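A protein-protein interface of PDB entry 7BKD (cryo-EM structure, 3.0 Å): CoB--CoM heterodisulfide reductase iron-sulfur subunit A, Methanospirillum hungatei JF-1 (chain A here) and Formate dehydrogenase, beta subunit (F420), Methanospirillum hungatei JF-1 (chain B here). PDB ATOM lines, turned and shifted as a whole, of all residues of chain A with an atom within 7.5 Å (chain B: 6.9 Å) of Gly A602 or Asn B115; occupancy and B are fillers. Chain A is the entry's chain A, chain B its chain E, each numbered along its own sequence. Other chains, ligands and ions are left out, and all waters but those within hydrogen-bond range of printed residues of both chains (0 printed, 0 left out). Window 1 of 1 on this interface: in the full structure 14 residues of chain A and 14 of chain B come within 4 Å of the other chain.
The side-chain amide nitrogen (NE2) of Gln B116 lies within hydrogen-bond range of the backbone carbonyl oxygen (O) of Ala A601, at 3.5 Å. O of Cys A603 sits at hydrogen-bond distance from ND2 of Asn B115 (2.8 Å). The side-chain hydroxyl (OH) of Tyr B307 sits close to the side-chain sulfur (SG) of Cys A603 (3.4 Å). The side-chain sulfur (SD) of Met A605 lies close to the side-chain hydroxyl (OH) of Tyr B307.
The side-chain sulfur of Cys A600 sits close to the backbone NH of Gly A602, at 3.2 Å. The guanidinium group (NH2) of Arg A623 sits at hydrogen-bond distance from the backbone carbonyl oxygen (O) of Cys A600 (2.6 Å). The backbone NH (N) of Met A626 sits close to the side-chain sulfur (SG) of Cys A600 (3.5 Å). The side-chain carboxylate (OE2) of Glu B110 is in salt-bridge range of the guanidinium group (NH1) of Arg B114 (3.0 Å). The backbone carbonyl oxygen of Leu B111 lies within hydrogen-bond range of the backbone NH of Gln B116 (3.0 Å). The side-chain amide nitrogen (NE2) of Gln B116 lies within hydrogen-bond range of the backbone carbonyl oxygen (O) of Arg B114, 3.0 Å away.
Among the printed residues, merely in contact across the chains: Leu A599 with Ile B309, Cys A600 with Ile B309, Ala A601 with Tyr B307, Gly A602 with Asn B115, Cys A603 with Arg B114 and Met A605 with Arg B114.
Of the printed residues of chain B, Ala A601 touches Gln B116 and Tyr B307. Leu B111 touches none of the printed residues of chain A. Of the printed residues of chain A, Arg B114 touches Cys A603 and Met A605. Asn B115 touches just these residues of chain A: Gly A602 (3.4 Å) and Cys A603 (2.8 Å). Printed residues of chain A within 4 Å of Gln B116: Ala A601 (3.5 Å). Printed residues of chain A within 4 Å of Tyr B307: Ala A601, Cys A603 and Met A605. The nearest residue of chain B that does not touch Gly A602 is Arg B114 (4.4 Å).
Printed residues of chain A that touch a printed residue of chain B: Leu A599, Cys A600, Ala A601, Gly A602, Cys A603 and Met A605. Along chain A the printed residues that touch a printed residue of chain B span positions 599 to 605. Hydrophobic or aromatic side chains of chain B within 4 Å of the printed part of chain A: Tyr B307 and Ile B309. Among the printed residues, no Asp or Glu carboxylate lies within 4 Å of a Lys or Arg side-chain nitrogen of the other chain.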
ATOM      1  N   ASP A 597      37.336 -20.318 -17.629  1.00  0.00           N
ATOM      2  CA  ASP A 597      36.617 -20.281 -16.362  1.00  0.00           C
ATOM      3  C   ASP A 597      37.485 -19.800 -15.208  1.00  0.00           C
ATOM      4  O   ASP A 597      36.951 -19.437 -14.157  1.00  0.00           O
ATOM      5  CB  ASP A 597      36.037 -21.657 -16.048  1.00  0.00           C
ATOM      6  CG  ASP A 597      37.069 -22.755 -16.132  1.00  0.00           C
ATOM      7  OD1 ASP A 597      38.182 -22.485 -16.627  1.00  0.00           O
ATOM      8  OD2 ASP A 597      36.769 -23.888 -15.702  1.00  0.00           O
ATOM      9  N   LEU A 599      38.940 -17.061 -15.324  1.00  0.00           N
ATOM     10  CA  LEU A 599      38.744 -15.622 -15.352  1.00  0.00           C
ATOM     11  C   LEU A 599      37.284 -15.211 -15.281  1.00  0.00           C
ATOM     12  O   LEU A 599      37.004 -14.019 -15.137  1.00  0.00           O
ATOM     13  CB  LEU A 599      39.369 -15.021 -16.615  1.00  0.00           C
ATOM     14  CG  LEU A 599      40.833 -15.354 -16.864  1.00  0.00           C
ATOM     15  CD1 LEU A 599      41.257 -14.840 -18.215  1.00  0.00           C
ATOM     16  CD2 LEU A 599      41.682 -14.737 -15.782  1.00  0.00           C
ATOM     17  N   CYS A 600      36.353 -16.150 -15.386  1.00  0.00           N
ATOM     18  CA  CYS A 600      34.947 -15.803 -15.277  1.00  0.00           C
ATOM     19  C   CYS A 600      34.602 -15.480 -13.835  1.00  0.00           C
ATOM     20  O   CYS A 600      35.125 -16.091 -12.903  1.00  0.00           O
ATOM     21  CB  CYS A 600      34.071 -16.944 -15.784  1.00  0.00           C
ATOM     22  SG  CYS A 600      32.303 -16.609 -15.735  1.00  0.00           S
ATOM     23  N   ALA A 601      33.722 -14.502 -13.653  1.00  0.00           N
ATOM     24  CA  ALA A 601      33.235 -14.126 -12.340  1.00  0.00           C
ATOM     25  C   ALA A 601      31.777 -14.491 -12.132  1.00  0.00           C
ATOM     26  O   ALA A 601      31.214 -14.152 -11.090  1.00  0.00           O
ATOM     27  CB  ALA A 601      33.423 -12.625 -12.112  1.00  0.00           C
ATOM     28  N   GLY A 602      31.151 -15.161 -13.091  1.00  0.00           N
ATOM     29  CA  GLY A 602      29.780 -15.592 -12.916  1.00  0.00           C
ATOM     30  C   GLY A 602      28.774 -14.473 -12.843  1.00  0.00           C
ATOM     31  O   GLY A 602      27.713 -14.644 -12.242  1.00  0.00           O
ATOM     32  N   CYS A 603      29.088 -13.319 -13.431  1.00  0.00           N
ATOM     33  CA  CYS A 603      28.136 -12.215 -13.447  1.00  0.00           C
ATOM     34  C   CYS A 603      26.896 -12.568 -14.252  1.00  0.00           C
ATOM     35  O   CYS A 603      25.772 -12.257 -13.847  1.00  0.00           O
ATOM     36  CB  CYS A 603      28.798 -10.962 -14.007  1.00  0.00           C
ATOM     37  SG  CYS A 603      28.991 -10.956 -15.786  1.00  0.00           S
ATOM     38  N   GLY A 604      27.079 -13.221 -15.393  1.00  0.00           N
ATOM     39  CA  GLY A 604      25.964 -13.624 -16.214  1.00  0.00           C
ATOM     40  C   GLY A 604      25.394 -12.550 -17.106  1.00  0.00           C
ATOM     41  O   GLY A 604      24.289 -12.731 -17.624  1.00  0.00           O
ATOM     42  N   MET A 605      26.093 -11.429 -17.290  1.00  0.00           N
ATOM     43  CA  MET A 605      25.583 -10.405 -18.193  1.00  0.00           C
ATOM     44  C   MET A 605      25.531 -10.911 -19.624  1.00  0.00           C
ATOM     45  O   MET A 605      24.564 -10.651 -20.349  1.00  0.00           O
ATOM     46  CB  MET A 605      26.440  -9.146 -18.141  1.00  0.00           C
ATOM     47  CG  MET A 605      26.515  -8.402 -16.830  1.00  0.00           C
ATOM     48  SD  MET A 605      27.926  -7.301 -17.011  1.00  0.00           S
ATOM     49  CE  MET A 605      28.100  -6.630 -15.390  1.00  0.00           C
ATOM     50  N   LEU A 617      24.744 -20.105 -17.647  1.00  0.00           N
ATOM     51  CA  LEU A 617      25.448 -19.979 -16.379  1.00  0.00           C
ATOM     52  C   LEU A 617      25.364 -21.308 -15.641  1.00  0.00           C
ATOM     53  O   LEU A 617      24.268 -21.756 -15.293  1.00  0.00           O
ATOM     54  CB  LEU A 617      24.838 -18.852 -15.548  1.00  0.00           C
ATOM     55  CG  LEU A 617      25.764 -18.042 -14.651  1.00  0.00           C
ATOM     56  CD1 LEU A 617      26.807 -17.343 -15.482  1.00  0.00           C
ATOM     57  CD2 LEU A 617      24.959 -17.036 -13.860  1.00  0.00           C
ATOM     58  N   GLY A 618      26.517 -21.933 -15.402  1.00  0.00           N
ATOM     59  CA  GLY A 618      26.542 -23.252 -14.809  1.00  0.00           C
ATOM     60  C   GLY A 618      27.711 -23.422 -13.861  1.00  0.00           C
ATOM     61  O   GLY A 618      28.694 -22.681 -13.904  1.00  0.00           O
ATOM     62  N   ARG A 623      32.265 -23.304  -8.474  1.00  0.00           N
ATOM     63  CA  ARG A 623      32.092 -21.905  -8.827  1.00  0.00           C
ATOM     64  C   ARG A 623      31.039 -21.782  -9.912  1.00  0.00           C
ATOM     65  O   ARG A 623      30.977 -22.610 -10.824  1.00  0.00           O
ATOM     66  CB  ARG A 623      33.403 -21.298  -9.323  1.00  0.00           C
ATOM     67  CG  ARG A 623      34.318 -20.797  -8.237  1.00  0.00           C
ATOM     68  CD  ARG A 623      35.652 -20.390  -8.821  1.00  0.00           C
ATOM     69  NE  ARG A 623      35.480 -19.606 -10.036  1.00  0.00           N
ATOM     70  CZ  ARG A 623      36.401 -18.795 -10.541  1.00  0.00           C
ATOM     71  NH1 ARG A 623      37.573 -18.660  -9.937  1.00  0.00           N
ATOM     72  NH2 ARG A 623      36.152 -18.122 -11.652  1.00  0.00           N
ATOM     73  N   THR A 624      30.212 -20.750  -9.813  1.00  0.00           N
ATOM     74  CA  THR A 624      29.272 -20.440 -10.879  1.00  0.00           C
ATOM     75  C   THR A 624      30.009 -19.701 -11.983  1.00  0.00           C
ATOM     76  O   THR A 624      30.516 -18.596 -11.770  1.00  0.00           O
ATOM     77  CB  THR A 624      28.113 -19.605 -10.353  1.00  0.00           C
ATOM     78  OG1 THR A 624      27.221 -20.445  -9.613  1.00  0.00           O
ATOM     79  CG2 THR A 624      27.360 -18.983 -11.500  1.00  0.00           C
ATOM     80  N   VAL A 625      30.094 -20.322 -13.154  1.00  0.00           N
ATOM     81  CA  VAL A 625      30.780 -19.763 -14.301  1.00  0.00           C
ATOM     82  C   VAL A 625      29.865 -19.863 -15.512  1.00  0.00           C
ATOM     83  O   VAL A 625      28.728 -20.320 -15.427  1.00  0.00           O
ATOM     84  CB  VAL A 625      32.124 -20.462 -14.581  1.00  0.00           C
ATOM     85  CG1 VAL A 625      33.050 -20.333 -13.399  1.00  0.00           C
ATOM     86  CG2 VAL A 625      31.889 -21.912 -14.921  1.00  0.00           C
ATOM     87  N   MET A 626      30.385 -19.426 -16.648  1.00  0.00           N
ATOM     88  CA  MET A 626      29.672 -19.479 -17.909  1.00  0.00           C
ATOM     89  C   MET A 626      30.057 -20.731 -18.683  1.00  0.00           C
ATOM     90  O   MET A 626      31.220 -21.142 -18.684  1.00  0.00           O
ATOM     91  CB  MET A 626      29.982 -18.248 -18.747  1.00  0.00           C
ATOM     92  CG  MET A 626      28.999 -18.031 -19.846  1.00  0.00           C
ATOM     93  SD  MET A 626      29.747 -18.612 -21.360  1.00  0.00           S
ATOM     94  CE  MET A 626      31.183 -17.566 -21.461  1.00  0.00           C
ATOM     95  N   LYS B  92      25.752 -15.625   0.417  1.00  0.00           N
ATOM     96  CA  LYS B  92      25.049 -16.697  -0.272  1.00  0.00           C
ATOM     97  C   LYS B  92      24.633 -17.818   0.665  1.00  0.00           C
ATOM     98  O   LYS B  92      23.832 -18.670   0.271  1.00  0.00           O
ATOM     99  CB  LYS B  92      25.921 -17.247  -1.398  1.00  0.00           C
ATOM    100  CG  LYS B  92      26.139 -16.239  -2.507  1.00  0.00           C
ATOM    101  CD  LYS B  92      26.958 -16.799  -3.649  1.00  0.00           C
ATOM    102  CE  LYS B  92      27.216 -15.721  -4.691  1.00  0.00           C
ATOM    103  NZ  LYS B  92      25.967 -15.305  -5.388  1.00  0.00           N
ATOM    104  N   GLU B 110      24.051  -2.407  -7.413  1.00  0.00           N
ATOM    105  CA  GLU B 110      24.996  -2.605  -8.506  1.00  0.00           C
ATOM    106  C   GLU B 110      25.685  -3.958  -8.409  1.00  0.00           C
ATOM    107  O   GLU B 110      25.961  -4.592  -9.431  1.00  0.00           O
ATOM    108  CB  GLU B 110      26.023  -1.478  -8.522  1.00  0.00           C
ATOM    109  CG  GLU B 110      25.529  -0.198  -9.161  1.00  0.00           C
ATOM    110  CD  GLU B 110      24.888  -0.427 -10.515  1.00  0.00           C
ATOM    111  OE1 GLU B 110      23.649  -0.396 -10.602  1.00  0.00           O
ATOM    112  OE2 GLU B 110      25.622  -0.630 -11.500  1.00  0.00           O
ATOM    113  N   LEU B 111      25.981  -4.415  -7.192  1.00  0.00           N
ATOM    114  CA  LEU B 111      26.577  -5.736  -7.032  1.00  0.00           C
ATOM    115  C   LEU B 111      25.556  -6.844  -7.238  1.00  0.00           C
ATOM    116  O   LEU B 111      25.919  -7.945  -7.656  1.00  0.00           O
ATOM    117  CB  LEU B 111      27.222  -5.858  -5.653  1.00  0.00           C
ATOM    118  CG  LEU B 111      28.546  -5.118  -5.468  1.00  0.00           C
ATOM    119  CD1 LEU B 111      28.782  -4.815  -4.014  1.00  0.00           C
ATOM    120  CD2 LEU B 111      29.693  -5.929  -6.025  1.00  0.00           C
ATOM    121  N   ALA B 112      24.284  -6.582  -6.940  1.00  0.00           N
ATOM    122  CA  ALA B 112      23.255  -7.584  -7.175  1.00  0.00           C
ATOM    123  C   ALA B 112      22.963  -7.760  -8.656  1.00  0.00           C
ATOM    124  O   ALA B 112      22.659  -8.873  -9.097  1.00  0.00           O
ATOM    125  CB  ALA B 112      21.978  -7.210  -6.435  1.00  0.00           C
ATOM    126  N   LYS B 113      23.030  -6.679  -9.435  1.00  0.00           N
ATOM    127  CA  LYS B 113      22.860  -6.804 -10.876  1.00  0.00           C
ATOM    128  C   LYS B 113      23.879  -7.758 -11.475  1.00  0.00           C
ATOM    129  O   LYS B 113      23.626  -8.364 -12.519  1.00  0.00           O
ATOM    130  CB  LYS B 113      22.989  -5.440 -11.545  1.00  0.00           C
ATOM    131  CG  LYS B 113      21.868  -4.492 -11.242  1.00  0.00           C
ATOM    132  CD  LYS B 113      22.143  -3.126 -11.828  1.00  0.00           C
ATOM    133  CE  LYS B 113      21.128  -2.117 -11.330  1.00  0.00           C
ATOM    134  NZ  LYS B 113      21.341  -0.779 -11.928  1.00  0.00           N
ATOM    135  N   ARG B 114      25.030  -7.905 -10.828  1.00  0.00           N
ATOM    136  CA  ARG B 114      26.153  -8.657 -11.364  1.00  0.00           C
ATOM    137  C   ARG B 114      26.339  -9.997 -10.670  1.00  0.00           C
ATOM    138  O   ARG B 114      27.426 -10.573 -10.734  1.00  0.00           O
ATOM    139  CB  ARG B 114      27.420  -7.817 -11.254  1.00  0.00           C
ATOM    140  CG  ARG B 114      27.381  -6.611 -12.142  1.00  0.00           C
ATOM    141  CD  ARG B 114      28.491  -5.630 -11.852  1.00  0.00           C
ATOM    142  NE  ARG B 114      28.568  -4.594 -12.876  1.00  0.00           N
ATOM    143  CZ  ARG B 114      27.783  -3.527 -12.925  1.00  0.00           C
ATOM    144  NH1 ARG B 114      26.844  -3.346 -12.015  1.00  0.00           N
ATOM    145  NH2 ARG B 114      27.933  -2.644 -13.896  1.00  0.00           N
ATOM    146  N   ASN B 115      25.308 -10.493  -9.990  1.00  0.00           N
ATOM    147  CA  ASN B 115      25.338 -11.781  -9.304  1.00  0.00           C
ATOM    148  C   ASN B 115      26.440 -11.861  -8.257  1.00  0.00           C
ATOM    149  O   ASN B 115      26.842 -12.957  -7.864  1.00  0.00           O
ATOM    150  CB  ASN B 115      25.485 -12.936 -10.297  1.00  0.00           C
ATOM    151  CG  ASN B 115      24.155 -13.474 -10.764  1.00  0.00           C
ATOM    152  OD1 ASN B 115      23.297 -13.821  -9.957  1.00  0.00           O
ATOM    153  ND2 ASN B 115      23.976 -13.546 -12.076  1.00  0.00           N
ATOM    154  N   GLN B 116      26.943 -10.722  -7.790  1.00  0.00           N
ATOM    155  CA  GLN B 116      28.038 -10.728  -6.832  1.00  0.00           C
ATOM    156  C   GLN B 116      27.568 -10.933  -5.403  1.00  0.00           C
ATOM    157  O   GLN B 116      28.318 -11.478  -4.588  1.00  0.00           O
ATOM    158  CB  GLN B 116      28.836  -9.430  -6.935  1.00  0.00           C
ATOM    159  CG  GLN B 116      29.635  -9.315  -8.212  1.00  0.00           C
ATOM    160  CD  GLN B 116      30.446 -10.557  -8.510  1.00  0.00           C
ATOM    161  OE1 GLN B 116      31.500 -10.776  -7.922  1.00  0.00           O
ATOM    162  NE2 GLN B 116      29.959 -11.377  -9.431  1.00  0.00           N
ATOM    163  N   ILE B 117      26.350 -10.505  -5.075  1.00  0.00           N
ATOM    164  CA  ILE B 117      25.747 -10.759  -3.776  1.00  0.00           C
ATOM    165  C   ILE B 117      24.327 -11.249  -3.999  1.00  0.00           C
ATOM    166  O   ILE B 117      23.762 -11.118  -5.086  1.00  0.00           O
ATOM    167  CB  ILE B 117      25.721  -9.519  -2.868  1.00  0.00           C
ATOM    168  CG1 ILE B 117      24.672  -8.549  -3.379  1.00  0.00           C
ATOM    169  CG2 ILE B 117      27.071  -8.838  -2.825  1.00  0.00           C
ATOM    170  CD1 ILE B 117      24.336  -7.503  -2.405  1.00  0.00           C
ATOM    171  N   ASN B 118      23.745 -11.808  -2.946  1.00  0.00           N
ATOM    172  CA  ASN B 118      22.375 -12.313  -2.969  1.00  0.00           C
ATOM    173  C   ASN B 118      21.510 -11.381  -2.125  1.00  0.00           C
ATOM    174  O   ASN B 118      21.536 -11.449  -0.895  1.00  0.00           O
ATOM    175  CB  ASN B 118      22.321 -13.745  -2.450  1.00  0.00           C
ATOM    176  CG  ASN B 118      21.025 -14.437  -2.791  1.00  0.00           C
ATOM    177  OD1 ASN B 118      20.194 -13.897  -3.517  1.00  0.00           O
ATOM    178  ND2 ASN B 118      20.842 -15.641  -2.270  1.00  0.00           N
ATOM    179  N   TYR B 307      34.151  -5.942 -10.670  1.00  0.00           N
ATOM    180  CA  TYR B 307      33.956  -7.251 -10.067  1.00  0.00           C
ATOM    181  C   TYR B 307      34.849  -8.318 -10.671  1.00  0.00           C
ATOM    182  O   TYR B 307      34.819  -9.462 -10.208  1.00  0.00           O
ATOM    183  CB  TYR B 307      32.509  -7.719 -10.235  1.00  0.00           C
ATOM    184  CG  TYR B 307      32.130  -7.863 -11.685  1.00  0.00           C
ATOM    185  CD1 TYR B 307      32.035  -9.109 -12.270  1.00  0.00           C
ATOM    186  CD2 TYR B 307      31.851  -6.756 -12.465  1.00  0.00           C
ATOM    187  CE1 TYR B 307      31.706  -9.244 -13.593  1.00  0.00           C
ATOM    188  CE2 TYR B 307      31.514  -6.883 -13.785  1.00  0.00           C
ATOM    189  CZ  TYR B 307      31.441  -8.129 -14.344  1.00  0.00           C
ATOM    190  OH  TYR B 307      31.100  -8.259 -15.665  1.00  0.00           O
ATOM    191  N   ILE B 309      37.611 -10.969 -12.153  1.00  0.00           N
ATOM    192  CA  ILE B 309      38.651 -11.770 -11.519  1.00  0.00           C
ATOM    193  C   ILE B 309      40.021 -11.163 -11.781  1.00  0.00           C
ATOM    194  O   ILE B 309      40.825 -10.984 -10.862  1.00  0.00           O
ATOM    195  CB  ILE B 309      38.578 -13.223 -12.012  1.00  0.00           C
ATOM    196  CG1 ILE B 309      37.258 -13.857 -11.594  1.00  0.00           C
ATOM    197  CG2 ILE B 309      39.733 -14.019 -11.474  1.00  0.00           C
ATOM    198  CD1 ILE B 309      36.975 -13.740 -10.131  1.00  0.00           C
ATOM    199  N   MET B 381      17.566  -3.114  -9.954  1.00  0.00           N
ATOM    200  CA  MET B 381      18.269  -4.203 -10.639  1.00  0.00           C
ATOM    201  C   MET B 381      17.904  -4.317 -12.117  1.00  0.00           C
ATOM    202  O   MET B 381      17.732  -5.414 -12.647  1.00  0.00           O
ATOM    203  CB  MET B 381      18.035  -5.542  -9.942  1.00  0.00           C
ATOM    204  CG  MET B 381      18.640  -5.651  -8.565  1.00  0.00           C
ATOM    205  SD  MET B 381      18.240  -7.226  -7.811  1.00  0.00           S
ATOM    206  CE  MET B 381      19.244  -8.304  -8.823  1.00  0.00           C
